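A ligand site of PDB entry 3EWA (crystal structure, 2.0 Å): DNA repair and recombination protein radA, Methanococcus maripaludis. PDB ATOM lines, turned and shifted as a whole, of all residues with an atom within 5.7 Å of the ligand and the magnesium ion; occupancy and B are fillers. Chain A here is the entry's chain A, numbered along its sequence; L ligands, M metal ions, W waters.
N of Thr 112 lies within hydrogen-bond range of O6 of the ligand (2.9 Å). An oxygen (O6) of the ligand is in hydrogen-bond range of the backbone NH (N) of Gln 113, at 2.7 Å. NE2 of Gln 113 lies close to O6 of the ligand (3.4 Å). The backbone NH of Lys 111 is in hydrogen-bond range of an oxygen (O5) of the ligand (3.1 Å). The side-chain amino group of Lys 111 lies within salt-bridge range of an oxygen (O5) of the ligand (2.7 Å). N4 of the ligand sits at hydrogen-bond distance from OE1 of Gln 161. The backbone NH (N) of Gly 110 lies within hydrogen-bond range of an oxygen (O5) of the ligand, at 3.2 Å. N of Ser 109 is in hydrogen-bond range of O5 of the ligand. The side-chain hydroxyl of Ser 109 is in hydrogen-bond range of an oxygen (O5) of the ligand.
OE1 of Gln 113 is in hydrogen-bond range of NE of Arg 158. The side-chain amino group (NZ) of Lys 111 is in hydrogen-bond range of the backbone carbonyl oxygen (O) of Met 106. The backbone carbonyl oxygen (O) of Gly 105 is in hydrogen-bond range of the side-chain amino group (NZ) of Lys 111 (3.0 Å). The side-chain amide oxygen of Gln 161 is in hydrogen-bond range of the guanidinium group of Arg 158, 2.7 Å away. The guanidinium group of Arg 296 lies within hydrogen-bond range of the backbone carbonyl oxygen of Gly 108, at 3.2 Å. NH1 of Arg 158 lies within hydrogen-bond range of O of Thr 316 (2.8 Å). The side-chain carboxylate of Glu 317 sits at hydrogen-bond distance from the side-chain hydroxyl of Thr 316 (3.4 Å). The side-chain carboxylate (OE2) of Glu 151 sits at hydrogen-bond distance from the side-chain amide nitrogen (NE2) of Gln 257 (3.0 Å).
N of Gly 108 lies close to N1 of the ligand, at 3.0 Å. N4 of the ligand lies close to NH2 of Arg 158 (3.2 Å). Merely in contact with the ligand: Met 106, Phe 107, Glu 151, Ile 315, Thr 316 and Glu 317. Hydrophobic or aromatic side chains that line the ligand: Phe 107 and Ile 315. Within 4 Å of the ligand: Met 106, Phe 107, Gly 108, Ser 109, Gly 110, Lys 111, Thr 112, Gln 113, Glu 151, Arg 158, Gln 161, Ile 315, Thr 316 and Glu 317. The nearest printed residue that does not touch the ligand is Arg 296 (4.1 Å).
Within 4 Å of the magnesium ion: Thr 112.
The magnesium ion is bound by an oxygen (O2) of the ligand (1.9 Å), water W7 (2.0 Å), the side-chain hydroxyl (OG1) of Thr 112 (2.1 Å), an oxygen (O4) of the ligand (2.1 Å), water W6 (2.1 Å) and water W2 (2.1 Å).
Water W2 lies within hydrogen-bond range of the side-chain carboxylate of Glu 151 and the side-chain hydroxyl of Thr 153. Water W5 bridges the side-chain carboxylate of Glu 151 (2.7 Å) and an oxygen (O3) of the ligand (3.0 Å). Water W4 lies within hydrogen-bond range of O1 of the ligand (2.9 Å), OE2 of Glu 151 (3.0 Å) and NE2 of Gln 257 (3.3 Å). Water W8 bridges NE2 of Gln 161 (2.7 Å) and N4 of the ligand (3.3 Å).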
ATOM      1  N   GLY A 105     -15.249   5.392 -23.249  1.00  0.00           N
ATOM      2  CA  GLY A 105     -14.175   5.206 -24.195  1.00  0.00           C
ATOM      3  C   GLY A 105     -13.143   4.240 -23.671  1.00  0.00           C
ATOM      4  O   GLY A 105     -13.184   3.842 -22.504  1.00  0.00           O
ATOM      5  N   MET A 106     -12.237   3.836 -24.547  1.00  0.00           N
ATOM      6  CA  MET A 106     -11.188   2.905 -24.171  1.00  0.00           C
ATOM      7  C   MET A 106     -10.162   3.621 -23.306  1.00  0.00           C
ATOM      8  O   MET A 106     -10.228   4.844 -23.113  1.00  0.00           O
ATOM      9  CB  MET A 106     -10.514   2.343 -25.415  1.00  0.00           C
ATOM     10  CG  MET A 106     -11.435   1.473 -26.256  1.00  0.00           C
ATOM     11  SD  MET A 106     -10.611   0.839 -27.723  1.00  0.00           S
ATOM     12  CE  MET A 106     -11.175   2.025 -28.967  1.00  0.00           C
ATOM     13  N   PHE A 107      -9.218   2.857 -22.781  1.00  0.00           N
ATOM     14  CA  PHE A 107      -8.178   3.428 -21.934  1.00  0.00           C
ATOM     15  C   PHE A 107      -7.444   4.511 -22.710  1.00  0.00           C
ATOM     16  O   PHE A 107      -7.314   4.444 -23.950  1.00  0.00           O
ATOM     17  CB  PHE A 107      -7.177   2.348 -21.542  1.00  0.00           C
ATOM     18  CG  PHE A 107      -6.187   2.030 -22.628  1.00  0.00           C
ATOM     19  CD1 PHE A 107      -4.977   2.715 -22.701  1.00  0.00           C
ATOM     20  CD2 PHE A 107      -6.476   1.077 -23.597  1.00  0.00           C
ATOM     21  CE1 PHE A 107      -4.078   2.478 -23.723  1.00  0.00           C
ATOM     22  CE2 PHE A 107      -5.587   0.825 -24.634  1.00  0.00           C
ATOM     23  CZ  PHE A 107      -4.378   1.520 -24.708  1.00  0.00           C
ATOM     24  N   GLY A 108      -6.974   5.517 -21.985  1.00  0.00           N
ATOM     25  CA  GLY A 108      -6.218   6.607 -22.590  1.00  0.00           C
ATOM     26  C   GLY A 108      -6.975   7.473 -23.578  1.00  0.00           C
ATOM     27  O   GLY A 108      -6.340   8.293 -24.256  1.00  0.00           O
ATOM     28  N   SER A 109      -8.295   7.327 -23.666  1.00  0.00           N
ATOM     29  CA  SER A 109      -9.057   8.140 -24.610  1.00  0.00           C
ATOM     30  C   SER A 109      -9.275   9.564 -24.107  1.00  0.00           C
ATOM     31  O   SER A 109      -9.671  10.447 -24.875  1.00  0.00           O
ATOM     32  CB  SER A 109     -10.410   7.477 -24.948  1.00  0.00           C
ATOM     33  OG  SER A 109     -11.199   7.241 -23.797  1.00  0.00           O
ATOM     34  N   GLY A 110      -9.020   9.782 -22.818  1.00  0.00           N
ATOM     35  CA  GLY A 110      -9.144  11.119 -22.254  1.00  0.00           C
ATOM     36  C   GLY A 110     -10.291  11.411 -21.288  1.00  0.00           C
ATOM     37  O   GLY A 110     -10.546  12.575 -20.982  1.00  0.00           O
ATOM     38  N   LYS A 111     -10.975  10.367 -20.823  1.00  0.00           N
ATOM     39  CA  LYS A 111     -12.090  10.538 -19.918  1.00  0.00           C
ATOM     40  C   LYS A 111     -11.682  11.291 -18.645  1.00  0.00           C
ATOM     41  O   LYS A 111     -12.331  12.266 -18.259  1.00  0.00           O
ATOM     42  CB  LYS A 111     -12.685   9.171 -19.543  1.00  0.00           C
ATOM     43  CG  LYS A 111     -13.149   8.342 -20.741  1.00  0.00           C
ATOM     44  CD  LYS A 111     -13.781   7.011 -20.313  1.00  0.00           C
ATOM     45  CE  LYS A 111     -12.770   6.086 -19.661  1.00  0.00           C
ATOM     46  NZ  LYS A 111     -11.705   5.680 -20.623  1.00  0.00           N
ATOM     47  N   THR A 112     -10.600  10.860 -18.003  1.00  0.00           N
ATOM     48  CA  THR A 112     -10.151  11.506 -16.777  1.00  0.00           C
ATOM     49  C   THR A 112      -9.586  12.901 -17.039  1.00  0.00           C
ATOM     50  O   THR A 112      -9.724  13.787 -16.191  1.00  0.00           O
ATOM     51  CB  THR A 112      -9.118  10.615 -16.025  1.00  0.00           C
ATOM     52  OG1 THR A 112      -9.781   9.429 -15.568  1.00  0.00           O
ATOM     53  CG2 THR A 112      -8.529  11.343 -14.808  1.00  0.00           C
ATOM     54  N   GLN A 113      -8.959  13.112 -18.195  1.00  0.00           N
ATOM     55  CA  GLN A 113      -8.413  14.429 -18.520  1.00  0.00           C
ATOM     56  C   GLN A 113      -9.541  15.446 -18.553  1.00  0.00           C
ATOM     57  O   GLN A 113      -9.440  16.533 -17.970  1.00  0.00           O
ATOM     58  CB  GLN A 113      -7.705  14.424 -19.894  1.00  0.00           C
ATOM     59  CG  GLN A 113      -6.455  13.558 -19.979  1.00  0.00           C
ATOM     60  CD  GLN A 113      -5.483  13.822 -18.853  1.00  0.00           C
ATOM     61  OE1 GLN A 113      -4.873  14.900 -18.762  1.00  0.00           O
ATOM     62  NE2 GLN A 113      -5.330  12.844 -17.962  1.00  0.00           N
ATOM     63  N   ILE A 114     -10.635  15.096 -19.229  1.00  0.00           N
ATOM     64  CA  ILE A 114     -11.785  16.007 -19.315  1.00  0.00           C
ATOM     65  C   ILE A 114     -12.320  16.329 -17.931  1.00  0.00           C
ATOM     66  O   ILE A 114     -12.632  17.492 -17.636  1.00  0.00           O
ATOM     67  CB  ILE A 114     -12.912  15.409 -20.181  1.00  0.00           C
ATOM     68  CG1 ILE A 114     -12.461  15.337 -21.644  1.00  0.00           C
ATOM     69  CG2 ILE A 114     -14.175  16.263 -20.046  1.00  0.00           C
ATOM     70  CD1 ILE A 114     -13.397  14.557 -22.539  1.00  0.00           C
ATOM     71  N   GLU A 151     -11.291   5.031  -8.878  1.00  0.00           N
ATOM     72  CA  GLU A 151     -10.179   4.206  -9.331  1.00  0.00           C
ATOM     73  C   GLU A 151      -8.856   4.679  -8.727  1.00  0.00           C
ATOM     74  O   GLU A 151      -7.855   3.980  -8.815  1.00  0.00           O
ATOM     75  CB  GLU A 151     -10.084   4.231 -10.863  1.00  0.00           C
ATOM     76  CG  GLU A 151     -11.432   4.137 -11.564  1.00  0.00           C
ATOM     77  CD  GLU A 151     -11.315   3.944 -13.070  1.00  0.00           C
ATOM     78  OE1 GLU A 151     -10.373   4.486 -13.666  1.00  0.00           O
ATOM     79  OE2 GLU A 151     -12.180   3.256 -13.654  1.00  0.00           O
ATOM     80  N   THR A 153      -7.394   7.659  -9.591  1.00  0.00           N
ATOM     81  CA  THR A 153      -6.618   8.355 -10.594  1.00  0.00           C
ATOM     82  C   THR A 153      -6.705   9.879 -10.528  1.00  0.00           C
ATOM     83  O   THR A 153      -6.294  10.553 -11.458  1.00  0.00           O
ATOM     84  CB  THR A 153      -6.985   7.917 -12.028  1.00  0.00           C
ATOM     85  OG1 THR A 153      -8.402   7.959 -12.181  1.00  0.00           O
ATOM     86  CG2 THR A 153      -6.477   6.490 -12.293  1.00  0.00           C
ATOM     87  N   ARG A 158      -1.994  17.401 -11.977  1.00  0.00           N
ATOM     88  CA  ARG A 158      -2.587  17.685 -13.282  1.00  0.00           C
ATOM     89  C   ARG A 158      -3.542  18.862 -13.207  1.00  0.00           C
ATOM     90  O   ARG A 158      -3.642  19.656 -14.130  1.00  0.00           O
ATOM     91  CB  ARG A 158      -3.301  16.427 -13.786  1.00  0.00           C
ATOM     92  CG  ARG A 158      -3.804  16.527 -15.211  1.00  0.00           C
ATOM     93  CD  ARG A 158      -2.713  16.904 -16.188  1.00  0.00           C
ATOM     94  NE  ARG A 158      -3.152  16.693 -17.565  1.00  0.00           N
ATOM     95  CZ  ARG A 158      -2.703  17.382 -18.614  1.00  0.00           C
ATOM     96  NH1 ARG A 158      -3.170  17.096 -19.822  1.00  0.00           N
ATOM     97  NH2 ARG A 158      -1.781  18.334 -18.465  1.00  0.00           N
ATOM     98  N   GLN A 161      -1.382  21.918 -13.060  1.00  0.00           N
ATOM     99  CA  GLN A 161      -0.790  22.111 -14.387  1.00  0.00           C
ATOM    100  C   GLN A 161      -1.815  22.689 -15.378  1.00  0.00           C
ATOM    101  O   GLN A 161      -1.514  23.633 -16.111  1.00  0.00           O
ATOM    102  CB  GLN A 161      -0.238  20.777 -14.899  1.00  0.00           C
ATOM    103  CG  GLN A 161       0.434  20.832 -16.254  1.00  0.00           C
ATOM    104  CD  GLN A 161       1.007  19.499 -16.668  1.00  0.00           C
ATOM    105  OE1 GLN A 161       0.305  18.487 -16.714  1.00  0.00           O
ATOM    106  NE2 GLN A 161       2.306  19.472 -16.977  1.00  0.00           N
ATOM    107  N   ASP A 211     -15.922   9.374 -11.471  1.00  0.00           N
ATOM    108  CA  ASP A 211     -14.909   8.789 -12.355  1.00  0.00           C
ATOM    109  C   ASP A 211     -14.195   7.677 -11.590  1.00  0.00           C
ATOM    110  O   ASP A 211     -13.374   7.969 -10.731  1.00  0.00           O
ATOM    111  CB  ASP A 211     -13.928   9.917 -12.727  1.00  0.00           C
ATOM    112  CG  ASP A 211     -12.797   9.460 -13.632  1.00  0.00           C
ATOM    113  OD1 ASP A 211     -13.013   8.561 -14.480  1.00  0.00           O
ATOM    114  OD2 ASP A 211     -11.684  10.033 -13.515  1.00  0.00           O
ATOM    115  N   GLN A 257     -16.305   2.936 -18.792  1.00  0.00           N
ATOM    116  CA  GLN A 257     -15.339   2.117 -19.522  1.00  0.00           C
ATOM    117  C   GLN A 257     -16.091   1.386 -20.624  1.00  0.00           C
ATOM    118  O   GLN A 257     -17.323   1.479 -20.721  1.00  0.00           O
ATOM    119  CB  GLN A 257     -14.676   1.116 -18.566  1.00  0.00           C
ATOM    120  CG  GLN A 257     -14.111   1.769 -17.298  1.00  0.00           C
ATOM    121  CD  GLN A 257     -13.243   0.836 -16.468  1.00  0.00           C
ATOM    122  OE1 GLN A 257     -13.591  -0.326 -16.239  1.00  0.00           O
ATOM    123  NE2 GLN A 257     -12.102   1.348 -16.000  1.00  0.00           N
ATOM    124  N   LYS A 290      -9.141   7.477 -29.643  1.00  0.00           N
ATOM    125  CA  LYS A 290      -7.856   8.086 -29.958  1.00  0.00           C
ATOM    126  C   LYS A 290      -7.602   8.204 -31.454  1.00  0.00           C
ATOM    127  O   LYS A 290      -8.082   7.398 -32.258  1.00  0.00           O
ATOM    128  CB  LYS A 290      -6.719   7.305 -29.299  1.00  0.00           C
ATOM    129  CG  LYS A 290      -6.842   7.234 -27.772  1.00  0.00           C
ATOM    130  CD  LYS A 290      -5.496   7.068 -27.079  1.00  0.00           C
ATOM    131  CE  LYS A 290      -4.946   5.653 -27.214  1.00  0.00           C
ATOM    132  NZ  LYS A 290      -3.683   5.503 -26.431  1.00  0.00           N
ATOM    133  N   ARG A 296      -7.719  13.453 -30.325  1.00  0.00           N
ATOM    134  CA  ARG A 296      -8.793  12.619 -29.801  1.00  0.00           C
ATOM    135  C   ARG A 296     -10.091  13.015 -30.508  1.00  0.00           C
ATOM    136  O   ARG A 296     -10.222  14.139 -30.981  1.00  0.00           O
ATOM    137  CB  ARG A 296      -8.944  12.839 -28.291  1.00  0.00           C
ATOM    138  CG  ARG A 296      -7.726  12.455 -27.456  1.00  0.00           C
ATOM    139  CD  ARG A 296      -7.602  10.953 -27.329  1.00  0.00           C
ATOM    140  NE  ARG A 296      -6.494  10.564 -26.441  1.00  0.00           N
ATOM    141  CZ  ARG A 296      -5.206  10.621 -26.781  1.00  0.00           C
ATOM    142  NH1 ARG A 296      -4.835  11.041 -27.983  1.00  0.00           N
ATOM    143  NH2 ARG A 296      -4.289  10.252 -25.903  1.00  0.00           N
ATOM    144  N   ILE A 315      -5.038  16.614 -26.239  1.00  0.00           N
ATOM    145  CA  ILE A 315      -4.703  16.569 -24.826  1.00  0.00           C
ATOM    146  C   ILE A 315      -3.232  16.933 -24.795  1.00  0.00           C
ATOM    147  O   ILE A 315      -2.393  16.195 -25.323  1.00  0.00           O
ATOM    148  CB  ILE A 315      -4.883  15.164 -24.227  1.00  0.00           C
ATOM    149  CG1 ILE A 315      -6.314  14.667 -24.446  1.00  0.00           C
ATOM    150  CG2 ILE A 315      -4.567  15.194 -22.735  1.00  0.00           C
ATOM    151  CD1 ILE A 315      -7.370  15.571 -23.842  1.00  0.00           C
ATOM    152  N   THR A 316      -2.919  18.084 -24.205  1.00  0.00           N
ATOM    153  CA  THR A 316      -1.533  18.542 -24.155  1.00  0.00           C
ATOM    154  C   THR A 316      -1.126  18.890 -22.735  1.00  0.00           C
ATOM    155  O   THR A 316      -1.856  18.625 -21.780  1.00  0.00           O
ATOM    156  CB  THR A 316      -1.347  19.808 -24.993  1.00  0.00           C
ATOM    157  OG1 THR A 316      -2.046  20.885 -24.363  1.00  0.00           O
ATOM    158  CG2 THR A 316      -1.892  19.613 -26.413  1.00  0.00           C
ATOM    159  N   GLU A 317       0.045  19.496 -22.605  1.00  0.00           N
ATOM    160  CA  GLU A 317       0.560  19.919 -21.308  1.00  0.00           C
ATOM    161  C   GLU A 317      -0.381  20.929 -20.677  1.00  0.00           C
ATOM    162  O   GLU A 317      -0.492  21.008 -19.442  1.00  0.00           O
ATOM    163  CB  GLU A 317       1.968  20.515 -21.466  1.00  0.00           C
ATOM    164  CG  GLU A 317       2.376  20.862 -22.912  1.00  0.00           C
ATOM    165  CD  GLU A 317       1.829  22.208 -23.399  1.00  0.00           C
ATOM    166  OE1 GLU A 317       2.175  23.261 -22.815  1.00  0.00           O
ATOM    167  OE2 GLU A 317       1.057  22.206 -24.392  1.00  0.00           O
HETATM  168  P1  LIG L   1      -8.749   5.106 -18.156  1.00  0.00           P
HETATM  169  O1  LIG L   1     -10.070   4.699 -18.530  1.00  0.00           O
HETATM  170  O2  LIG L   1      -8.841   5.745 -16.814  1.00  0.00           O
HETATM  171  O3  LIG L   1      -7.999   3.880 -18.160  1.00  0.00           O
HETATM  172  P2  LIG L   1      -8.735   7.599 -19.595  1.00  0.00           P
HETATM  173  O4  LIG L   1      -9.513   8.137 -18.446  1.00  0.00           O
HETATM  174  O5  LIG L   1      -9.715   7.538 -20.676  1.00  0.00           O
HETATM  175  N1  LIG L   1      -8.261   6.105 -19.388  1.00  0.00           N
HETATM  176  P3  LIG L   1      -6.823   9.682 -19.334  1.00  0.00           P
HETATM  177  O6  LIG L   1      -7.851  10.779 -19.034  1.00  0.00           O
HETATM  178  O7  LIG L   1      -6.235   9.151 -18.077  1.00  0.00           O
HETATM  179  O8  LIG L   1      -7.532   8.500 -20.142  1.00  0.00           O
HETATM  180  O9  LIG L   1      -5.663  10.327 -20.314  1.00  0.00           O
HETATM  181  C1  LIG L   1      -4.382   9.599 -20.664  1.00  0.00           C
HETATM  182  C2  LIG L   1      -3.701  10.329 -21.574  1.00  0.00           C
HETATM  183  O10 LIG L   1      -3.624  11.737 -21.122  1.00  0.00           O
HETATM  184  C3  LIG L   1      -2.209   9.888 -21.567  1.00  0.00           C
HETATM  185  O11 LIG L   1      -1.952   8.611 -22.029  1.00  0.00           O
HETATM  186  C4  LIG L   1      -1.391  11.162 -21.907  1.00  0.00           C
HETATM  187  O12 LIG L   1      -1.108  11.169 -23.414  1.00  0.00           O
HETATM  188  C5  LIG L   1      -2.360  12.305 -21.573  1.00  0.00           C
HETATM  189  N2  LIG L   1      -1.797  13.047 -20.582  1.00  0.00           N
HETATM  190  C6  LIG L   1      -1.910  12.856 -19.201  1.00  0.00           C
HETATM  191  N3  LIG L   1      -1.215  13.763 -18.577  1.00  0.00           N
HETATM  192  C7  LIG L   1      -0.635  14.570 -19.490  1.00  0.00           C
HETATM  193  C8  LIG L   1       0.187  15.689 -19.409  1.00  0.00           C
HETATM  194  N4  LIG L   1       0.590  16.171 -18.202  1.00  0.00           N
HETATM  195  N5  LIG L   1       0.619  16.308 -20.589  1.00  0.00           N
HETATM  196  C9  LIG L   1       0.230  15.815 -21.865  1.00  0.00           C
HETATM  197  N6  LIG L   1      -0.579  14.733 -21.979  1.00  0.00           N
HETATM  198  C10 LIG L   1      -0.993  14.135 -20.755  1.00  0.00           C
HETATM  199 MG    MG M   1      -9.493   7.526 -16.416  1.00  0.00          MG
HETATM  200  O   HOH W   1      -5.094   6.559 -18.736  1.00  0.00           O
HETATM  201  O   HOH W   2      -9.478   6.740 -14.431  1.00  0.00           O
HETATM  202  O   HOH W   3      -5.110   3.146 -17.999  1.00  0.00           O
HETATM  203  O   HOH W   4     -11.926   4.598 -16.322  1.00  0.00           O
HETATM  204  O   HOH W   5      -8.151   3.916 -15.161  1.00  0.00           O
HETATM  205  O   HOH W   6     -11.614   7.303 -16.324  1.00  0.00           O
HETATM  206  O   HOH W   7      -7.511   7.666 -16.134  1.00  0.00           O
HETATM  207  O   HOH W   8       3.617  17.518 -18.198  1.00  0.00           O
